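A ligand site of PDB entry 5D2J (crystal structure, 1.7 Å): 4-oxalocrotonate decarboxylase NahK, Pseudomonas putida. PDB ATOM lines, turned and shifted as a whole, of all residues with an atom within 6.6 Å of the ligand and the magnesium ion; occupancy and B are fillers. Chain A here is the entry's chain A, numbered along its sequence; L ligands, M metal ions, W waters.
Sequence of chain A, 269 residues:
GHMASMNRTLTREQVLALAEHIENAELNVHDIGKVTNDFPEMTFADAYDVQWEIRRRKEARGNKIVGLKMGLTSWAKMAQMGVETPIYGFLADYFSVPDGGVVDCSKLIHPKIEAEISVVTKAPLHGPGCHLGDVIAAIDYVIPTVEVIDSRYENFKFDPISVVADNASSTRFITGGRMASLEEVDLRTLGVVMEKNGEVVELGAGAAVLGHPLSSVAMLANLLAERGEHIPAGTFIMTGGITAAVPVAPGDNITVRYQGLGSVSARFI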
ATOM      1  N   LYS A  69      27.539  17.045  17.960  1.00  0.00           N
ATOM      2  CA  LYS A  69      26.658  15.891  17.821  1.00  0.00           C
ATOM      3  C   LYS A  69      27.458  14.601  17.808  1.00  0.00           C
ATOM      4  O   LYS A  69      28.642  14.605  17.498  1.00  0.00           O
ATOM      5  CB  LYS A  69      25.763  15.990  16.575  1.00  0.00           C
ATOM      6  CG  LYS A  69      26.452  16.370  15.270  1.00  0.00           C
ATOM      7  CD  LYS A  69      26.910  15.155  14.444  1.00  0.00           C
ATOM      8  CE  LYS A  69      25.776  14.169  14.134  1.00  0.00           C
ATOM      9  NZ  LYS A  69      25.064  14.379  12.818  1.00  0.00           N
ATOM     10  N   MET A  70      26.799  13.516  18.165  1.00  0.00           N
ATOM     11  CA  MET A  70      27.413  12.196  18.107  1.00  0.00           C
ATOM     12  C   MET A  70      26.682  11.361  17.067  1.00  0.00           C
ATOM     13  O   MET A  70      25.451  11.388  16.998  1.00  0.00           O
ATOM     14  CB  MET A  70      27.335  11.520  19.485  1.00  0.00           C
ATOM     15  CG  MET A  70      28.331  12.095  20.474  1.00  0.00           C
ATOM     16  SD  MET A  70      30.006  11.486  20.185  1.00  0.00           S
ATOM     17  CE  MET A  70      29.857   9.885  20.951  1.00  0.00           C
ATOM     18  N   GLY A  71      27.443  10.634  16.269  1.00  0.00           N
ATOM     19  CA  GLY A  71      26.880   9.759  15.260  1.00  0.00           C
ATOM     20  C   GLY A  71      27.425   8.340  15.336  1.00  0.00           C
ATOM     21  O   GLY A  71      28.434   8.102  16.007  1.00  0.00           O
ATOM     22  N   LEU A  72      26.752   7.420  14.658  1.00  0.00           N
ATOM     23  CA  LEU A  72      27.100   5.997  14.722  1.00  0.00           C
ATOM     24  C   LEU A  72      27.071   5.529  16.171  1.00  0.00           C
ATOM     25  O   LEU A  72      28.010   4.889  16.659  1.00  0.00           O
ATOM     26  CB  LEU A  72      28.467   5.722  14.078  1.00  0.00           C
ATOM     27  CG  LEU A  72      28.705   6.327  12.687  1.00  0.00           C
ATOM     28  CD1 LEU A  72      29.982   5.767  12.059  1.00  0.00           C
ATOM     29  CD2 LEU A  72      27.514   6.112  11.764  1.00  0.00           C
ATOM     30  N   THR A  73      25.992   5.842  16.867  1.00  0.00           N
ATOM     31  CA  THR A  73      25.863   5.515  18.272  1.00  0.00           C
ATOM     32  C   THR A  73      25.092   4.207  18.502  1.00  0.00           C
ATOM     33  O   THR A  73      24.683   3.916  19.618  1.00  0.00           O
ATOM     34  CB  THR A  73      25.202   6.659  19.062  1.00  0.00           C
ATOM     35  OG1 THR A  73      23.946   7.002  18.442  1.00  0.00           O
ATOM     36  CG2 THR A  73      26.091   7.897  19.078  1.00  0.00           C
ATOM     37  N   LYS A  77      25.083   0.386  13.792  1.00  0.00           N
ATOM     38  CA  LYS A  77      25.661   1.471  13.004  1.00  0.00           C
ATOM     39  C   LYS A  77      27.172   1.369  12.886  1.00  0.00           C
ATOM     40  O   LYS A  77      27.725   1.506  11.793  1.00  0.00           O
ATOM     41  CB  LYS A  77      25.251   2.817  13.596  1.00  0.00           C
ATOM     42  CG  LYS A  77      24.103   3.502  12.872  1.00  0.00           C
ATOM     43  CD  LYS A  77      24.573   4.094  11.548  1.00  0.00           C
ATOM     44  CE  LYS A  77      23.527   5.004  10.917  1.00  0.00           C
ATOM     45  NZ  LYS A  77      24.052   5.729   9.719  1.00  0.00           N
ATOM     46  N   MET A  81      29.712   0.437   9.474  1.00  0.00           N
ATOM     47  CA  MET A  81      30.761   1.360   9.083  1.00  0.00           C
ATOM     48  C   MET A  81      32.162   0.808   9.365  1.00  0.00           C
ATOM     49  O   MET A  81      33.166   1.468   9.082  1.00  0.00           O
ATOM     50  CB  MET A  81      30.560   2.708   9.788  1.00  0.00           C
ATOM     51  CG  MET A  81      29.278   3.434   9.401  1.00  0.00           C
ATOM     52  SD  MET A  81      29.426   4.321   7.836  1.00  0.00           S
ATOM     53  CE  MET A  81      27.704   4.729   7.521  1.00  0.00           C
ATOM     54  N   ILE A  87      31.333   8.642  16.018  1.00  0.00           N
ATOM     55  CA  ILE A  87      32.023   9.804  15.485  1.00  0.00           C
ATOM     56  C   ILE A  87      31.284  11.024  15.999  1.00  0.00           C
ATOM     57  O   ILE A  87      30.161  10.932  16.495  1.00  0.00           O
ATOM     58  CB  ILE A  87      32.035   9.814  13.944  1.00  0.00           C
ATOM     59  CG1 ILE A  87      30.608   9.838  13.389  1.00  0.00           C
ATOM     60  CG2 ILE A  87      32.777   8.597  13.400  1.00  0.00           C
ATOM     61  CD1 ILE A  87      30.537   9.991  11.846  1.00  0.00           C
ATOM     62  N   LYS A 112      17.160  13.482   5.692  1.00  0.00           N
ATOM     63  CA  LYS A 112      16.419  12.525   6.501  1.00  0.00           C
ATOM     64  C   LYS A 112      16.337  13.089   7.907  1.00  0.00           C
ATOM     65  O   LYS A 112      17.138  13.936   8.271  1.00  0.00           O
ATOM     66  CB  LYS A 112      17.137  11.183   6.562  1.00  0.00           C
ATOM     67  CG  LYS A 112      17.203  10.411   5.264  1.00  0.00           C
ATOM     68  CD  LYS A 112      17.865   9.072   5.483  1.00  0.00           C
ATOM     69  CE  LYS A 112      18.242   8.426   4.155  1.00  0.00           C
ATOM     70  NZ  LYS A 112      18.770   7.055   4.376  1.00  0.00           N
ATOM     71  N   GLU A 114      16.016  12.164  12.248  1.00  0.00           N
ATOM     72  CA  GLU A 114      16.240  11.203  13.334  1.00  0.00           C
ATOM     73  C   GLU A 114      15.779  11.896  14.597  1.00  0.00           C
ATOM     74  O   GLU A 114      16.100  13.066  14.796  1.00  0.00           O
ATOM     75  CB  GLU A 114      17.731  10.956  13.574  1.00  0.00           C
ATOM     76  CG  GLU A 114      18.589  10.493  12.430  1.00  0.00           C
ATOM     77  CD  GLU A 114      20.044  10.316  12.855  1.00  0.00           C
ATOM     78  OE1 GLU A 114      20.751  11.336  13.085  1.00  0.00           O
ATOM     79  OE2 GLU A 114      20.470   9.157  12.991  1.00  0.00           O
ATOM     80  N   GLU A 116      16.267  12.451  18.577  1.00  0.00           N
ATOM     81  CA  GLU A 116      17.368  12.308  19.520  1.00  0.00           C
ATOM     82  C   GLU A 116      17.013  13.019  20.821  1.00  0.00           C
ATOM     83  O   GLU A 116      15.994  13.706  20.900  1.00  0.00           O
ATOM     84  CB  GLU A 116      18.666  12.907  18.938  1.00  0.00           C
ATOM     85  CG  GLU A 116      18.911  12.520  17.478  1.00  0.00           C
ATOM     86  CD  GLU A 116      20.351  12.668  17.029  1.00  0.00           C
ATOM     87  OE1 GLU A 116      21.215  13.010  17.856  1.00  0.00           O
ATOM     88  OE2 GLU A 116      20.615  12.400  15.835  1.00  0.00           O
ATOM     89  N   GLU A 147      17.125  15.689  14.549  1.00  0.00           N
ATOM     90  CA  GLU A 147      18.195  16.080  13.639  1.00  0.00           C
ATOM     91  C   GLU A 147      17.738  15.920  12.209  1.00  0.00           C
ATOM     92  O   GLU A 147      17.023  14.981  11.882  1.00  0.00           O
ATOM     93  CB  GLU A 147      19.483  15.261  13.821  1.00  0.00           C
ATOM     94  CG  GLU A 147      20.677  15.957  13.117  1.00  0.00           C
ATOM     95  CD  GLU A 147      22.017  15.273  13.290  1.00  0.00           C
ATOM     96  OE1 GLU A 147      22.064  14.119  13.761  1.00  0.00           O
ATOM     97  OE2 GLU A 147      23.037  15.894  12.910  1.00  0.00           O
ATOM     98  N   ILE A 149      19.656  15.120   8.978  1.00  0.00           N
ATOM     99  CA  ILE A 149      20.968  14.749   8.443  1.00  0.00           C
ATOM    100  C   ILE A 149      20.931  14.768   6.917  1.00  0.00           C
ATOM    101  O   ILE A 149      19.899  14.477   6.295  1.00  0.00           O
ATOM    102  CB  ILE A 149      21.470  13.375   8.940  1.00  0.00           C
ATOM    103  CG1 ILE A 149      20.386  12.307   8.807  1.00  0.00           C
ATOM    104  CG2 ILE A 149      21.967  13.486  10.384  1.00  0.00           C
ATOM    105  CD1 ILE A 149      20.892  10.891   9.029  1.00  0.00           C
ATOM    106  N   ASP A 150      22.058  15.099   6.301  1.00  0.00           N
ATOM    107  CA  ASP A 150      22.043  15.306   4.863  1.00  0.00           C
ATOM    108  C   ASP A 150      23.458  15.201   4.340  1.00  0.00           C
ATOM    109  O   ASP A 150      24.128  16.212   4.141  1.00  0.00           O
ATOM    110  CB  ASP A 150      21.478  16.707   4.569  1.00  0.00           C
ATOM    111  CG  ASP A 150      21.158  16.913   3.109  1.00  0.00           C
ATOM    112  OD1 ASP A 150      20.766  15.936   2.437  1.00  0.00           O
ATOM    113  OD2 ASP A 150      21.302  18.062   2.619  1.00  0.00           O
ATOM    114  N   SER A 151      23.922  13.973   4.140  1.00  0.00           N
ATOM    115  CA  SER A 151      25.288  13.740   3.687  1.00  0.00           C
ATOM    116  C   SER A 151      25.533  14.447   2.366  1.00  0.00           C
ATOM    117  O   SER A 151      24.705  14.403   1.457  1.00  0.00           O
ATOM    118  CB  SER A 151      25.543  12.243   3.508  1.00  0.00           C
ATOM    119  OG  SER A 151      26.816  11.996   2.924  1.00  0.00           O
ATOM    120  N   PHE A 156      24.327   8.503  -0.752  1.00  0.00           N
ATOM    121  CA  PHE A 156      24.865   8.000   0.494  1.00  0.00           C
ATOM    122  C   PHE A 156      25.980   6.980   0.238  1.00  0.00           C
ATOM    123  O   PHE A 156      26.234   6.092   1.057  1.00  0.00           O
ATOM    124  CB  PHE A 156      23.741   7.456   1.369  1.00  0.00           C
ATOM    125  CG  PHE A 156      22.550   8.368   1.444  1.00  0.00           C
ATOM    126  CD1 PHE A 156      22.594   9.545   2.180  1.00  0.00           C
ATOM    127  CD2 PHE A 156      21.378   8.066   0.749  1.00  0.00           C
ATOM    128  CE1 PHE A 156      21.506  10.395   2.234  1.00  0.00           C
ATOM    129  CE2 PHE A 156      20.285   8.912   0.796  1.00  0.00           C
ATOM    130  CZ  PHE A 156      20.341  10.081   1.542  1.00  0.00           C
ATOM    131  N   PHE A 158      29.264   6.405   0.683  1.00  0.00           N
ATOM    132  CA  PHE A 158      30.387   6.928   1.455  1.00  0.00           C
ATOM    133  C   PHE A 158      31.131   5.895   2.325  1.00  0.00           C
ATOM    134  O   PHE A 158      30.932   4.685   2.160  1.00  0.00           O
ATOM    135  CB  PHE A 158      29.926   8.115   2.312  1.00  0.00           C
ATOM    136  CG  PHE A 158      28.670   7.866   3.101  1.00  0.00           C
ATOM    137  CD1 PHE A 158      28.532   6.749   3.907  1.00  0.00           C
ATOM    138  CD2 PHE A 158      27.632   8.789   3.065  1.00  0.00           C
ATOM    139  CE1 PHE A 158      27.380   6.537   4.643  1.00  0.00           C
ATOM    140  CE2 PHE A 158      26.474   8.590   3.798  1.00  0.00           C
ATOM    141  CZ  PHE A 158      26.347   7.460   4.590  1.00  0.00           C
ATOM    142  N   VAL A 163      32.711  10.549   5.897  1.00  0.00           N
ATOM    143  CA  VAL A 163      31.609  11.108   6.676  1.00  0.00           C
ATOM    144  C   VAL A 163      32.107  12.048   7.771  1.00  0.00           C
ATOM    145  O   VAL A 163      31.523  13.122   7.984  1.00  0.00           O
ATOM    146  CB  VAL A 163      30.719   9.985   7.254  1.00  0.00           C
ATOM    147  CG1 VAL A 163      29.743  10.524   8.298  1.00  0.00           C
ATOM    148  CG2 VAL A 163      29.982   9.312   6.108  1.00  0.00           C
ATOM    149  N   ASN A 167      31.609  16.484   8.364  1.00  0.00           N
ATOM    150  CA  ASN A 167      30.977  16.915   9.617  1.00  0.00           C
ATOM    151  C   ASN A 167      29.816  16.009  10.033  1.00  0.00           C
ATOM    152  O   ASN A 167      28.807  16.485  10.543  1.00  0.00           O
ATOM    153  CB  ASN A 167      30.509  18.374   9.532  1.00  0.00           C
ATOM    154  CG  ASN A 167      30.167  18.949  10.892  1.00  0.00           C
ATOM    155  OD1 ASN A 167      30.771  18.568  11.898  1.00  0.00           O
ATOM    156  ND2 ASN A 167      29.208  19.876  10.935  1.00  0.00           N
ATOM    157  N   ALA A 168      29.971  14.721   9.782  1.00  0.00           N
ATOM    158  CA  ALA A 168      28.985  13.715  10.167  1.00  0.00           C
ATOM    159  C   ALA A 168      27.593  14.034   9.627  1.00  0.00           C
ATOM    160  O   ALA A 168      26.599  13.799  10.310  1.00  0.00           O
ATOM    161  CB  ALA A 168      28.927  13.578  11.693  1.00  0.00           C
ATOM    162  N   SER A 169      27.526  14.583   8.410  1.00  0.00           N
ATOM    163  CA  SER A 169      26.250  14.824   7.717  1.00  0.00           C
ATOM    164  C   SER A 169      25.334  15.864   8.378  1.00  0.00           C
ATOM    165  O   SER A 169      24.149  15.947   8.042  1.00  0.00           O
ATOM    166  CB  SER A 169      25.469  13.513   7.551  1.00  0.00           C
ATOM    167  OG  SER A 169      26.256  12.519   6.895  1.00  0.00           O
ATOM    168  N   SER A 170      25.880  16.653   9.302  1.00  0.00           N
ATOM    169  CA  SER A 170      25.089  17.661   9.993  1.00  0.00           C
ATOM    170  C   SER A 170      24.560  18.760   9.071  1.00  0.00           C
ATOM    171  O   SER A 170      25.266  19.205   8.161  1.00  0.00           O
ATOM    172  CB  SER A 170      25.909  18.307  11.112  1.00  0.00           C
ATOM    173  OG  SER A 170      26.429  17.310  11.965  1.00  0.00           O
ATOM    174  N   MET A 238      23.984  16.827  20.998  1.00  0.00           N
ATOM    175  CA  MET A 238      22.973  15.907  20.457  1.00  0.00           C
ATOM    176  C   MET A 238      23.538  14.500  20.539  1.00  0.00           C
ATOM    177  O   MET A 238      24.505  14.174  19.846  1.00  0.00           O
ATOM    178  CB  MET A 238      22.640  16.265  19.010  1.00  0.00           C
ATOM    179  CG  MET A 238      21.931  17.588  18.874  1.00  0.00           C
ATOM    180  SD  MET A 238      21.401  17.857  17.183  1.00  0.00           S
ATOM    181  CE  MET A 238      20.528  16.324  16.914  1.00  0.00           C
ATOM    182  N   THR A 239      22.940  13.664  21.381  1.00  0.00           N
ATOM    183  CA  THR A 239      23.618  12.432  21.781  1.00  0.00           C
ATOM    184  C   THR A 239      23.563  11.245  20.842  1.00  0.00           C
ATOM    185  O   THR A 239      24.332  10.300  21.008  1.00  0.00           O
ATOM    186  CB  THR A 239      23.219  11.975  23.205  1.00  0.00           C
ATOM    187  OG1 THR A 239      21.807  11.714  23.257  1.00  0.00           O
ATOM    188  CG2 THR A 239      23.567  13.072  24.227  1.00  0.00           C
ATOM    189  N   GLY A 240      22.663  11.283  19.852  1.00  0.00           N
ATOM    190  CA  GLY A 240      22.590  10.209  18.872  1.00  0.00           C
ATOM    191  C   GLY A 240      21.178   9.791  18.477  1.00  0.00           C
ATOM    192  O   GLY A 240      20.219  10.069  19.194  1.00  0.00           O
ATOM    193  N   GLY A 241      21.064   9.098  17.350  1.00  0.00           N
ATOM    194  CA  GLY A 241      19.758   8.683  16.855  1.00  0.00           C
ATOM    195  C   GLY A 241      19.063   7.652  17.731  1.00  0.00           C
ATOM    196  O   GLY A 241      19.586   6.550  17.955  1.00  0.00           O
ATOM    197  N   ALA A 245      16.568   6.733  10.716  1.00  0.00           N
ATOM    198  CA  ALA A 245      16.419   7.949   9.925  1.00  0.00           C
ATOM    199  C   ALA A 245      15.336   7.790   8.839  1.00  0.00           C
ATOM    200  O   ALA A 245      15.215   6.739   8.230  1.00  0.00           O
ATOM    201  CB  ALA A 245      17.744   8.342   9.313  1.00  0.00           C
HETATM  202  O1  LIG L   1      24.307   9.572  13.208  1.00  0.00           O
HETATM  203  C1  LIG L   1      24.508  10.712  12.724  1.00  0.00           C
HETATM  204  O2  LIG L   1      23.878  11.701  13.181  1.00  0.00           O
HETATM  205  C2  LIG L   1      25.500  10.905  11.595  1.00  0.00           C
HETATM  206  C3  LIG L   1      25.200   9.942  10.460  1.00  0.00           C
HETATM  207  C4  LIG L   1      26.132  10.219   9.307  1.00  0.00           C
HETATM  208  C5  LIG L   1      25.976   9.188   8.208  1.00  0.00           C
HETATM  209  C6  LIG L   1      24.701   9.408   7.419  1.00  0.00           C
HETATM  210  O3  LIG L   1      24.541  10.476   6.765  1.00  0.00           O
HETATM  211  O4  LIG L   1      23.795   8.521   7.393  1.00  0.00           O
HETATM  212 MG    MG M   1      22.186  12.152  14.508  1.00  0.00          MG
HETATM  213  O   HOH W   1      22.005   8.476   5.100  1.00  0.00           O
HETATM  214  O   HOH W   2      22.637  11.286   5.157  1.00  0.00           O
HETATM  215  O   HOH W   3      23.327  12.852  16.215  1.00  0.00           O
HETATM  216  O   HOH W   4      22.484  10.061  14.953  1.00  0.00           O
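The magnesium ion is bound by OE2 of Glu 116, OE1 of Glu 147, water W4, water W3, OE1 of Glu 114 and O2 of the ligand. The magnesium ion has six donor atoms within binding distance.
The nearest printed residue that does not touch the magnesium ion is Lys 69 (4.01 Å).
The side-chain amino group of Lys 77 lies within salt-bridge range of an oxygen (O4) of the ligand (3.6 Å). The side-chain amino group of Lys 69 lies close to an oxygen (O2) of the ligand, at 3.0 Å. OG of Ser 169 lies within hydrogen-bond range of O3 of the ligand.
Water W3 bridges OE1 of Glu 116 and O of Met 70. Water W4 lies within hydrogen-bond range of an oxygen (O1) of the ligand (2.6 Å), the backbone NH of Gly 241 (2.9 Å) and the side-chain carboxylate of Glu 114 (3.0 Å). Water W2 lies within hydrogen-bond range of O3 of the ligand (2.6 Å) and N of Ser 151 (3.1 Å).
N of Ile 149 is in hydrogen-bond range of O of Lys 112 (2.9 Å). O of Ala 168 lies within hydrogen-bond range of NZ of Lys 69, at 3.0 Å. The backbone carbonyl oxygen (O) of Val 163 sits at hydrogen-bond distance from the backbone NH (N) of Ala 168 (2.9 Å). The backbone carbonyl oxygen (O) of Ile 87 lies within hydrogen-bond range of the backbone NH (N) of Gly 71, 2.7 Å away. O of Ser 169 lies within hydrogen-bond range of N of Asp 150 (2.8 Å). NZ of Lys 69 lies within salt-bridge range of OE2 of Glu 147. The side-chain amino group (NZ) of Lys 69 lies close to the side-chain hydroxyl (OG) of Ser 170 (3.3 Å). OE1 of Glu 116 is in hydrogen-bond range of N of Gly 240, at 3.0 Å.
Gly 71 touches the ligand (CA to O1, 3.3 Å). N of Leu 72 touches O1 of the ligand, 3.6 Å away. Ile 149 touches the ligand. Ser 151 touches the ligand (CB to O3, 3.8 Å). Phe 158 touches the ligand. CG1 of Val 163 touches C4 of the ligand, 3.8 Å away. Ala 168 touches the ligand. Of the 27 residues printed, 12 come within 4 Å of the ligand. The nearest printed residue that does not touch the ligand is Met 70 (4.1 Å).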
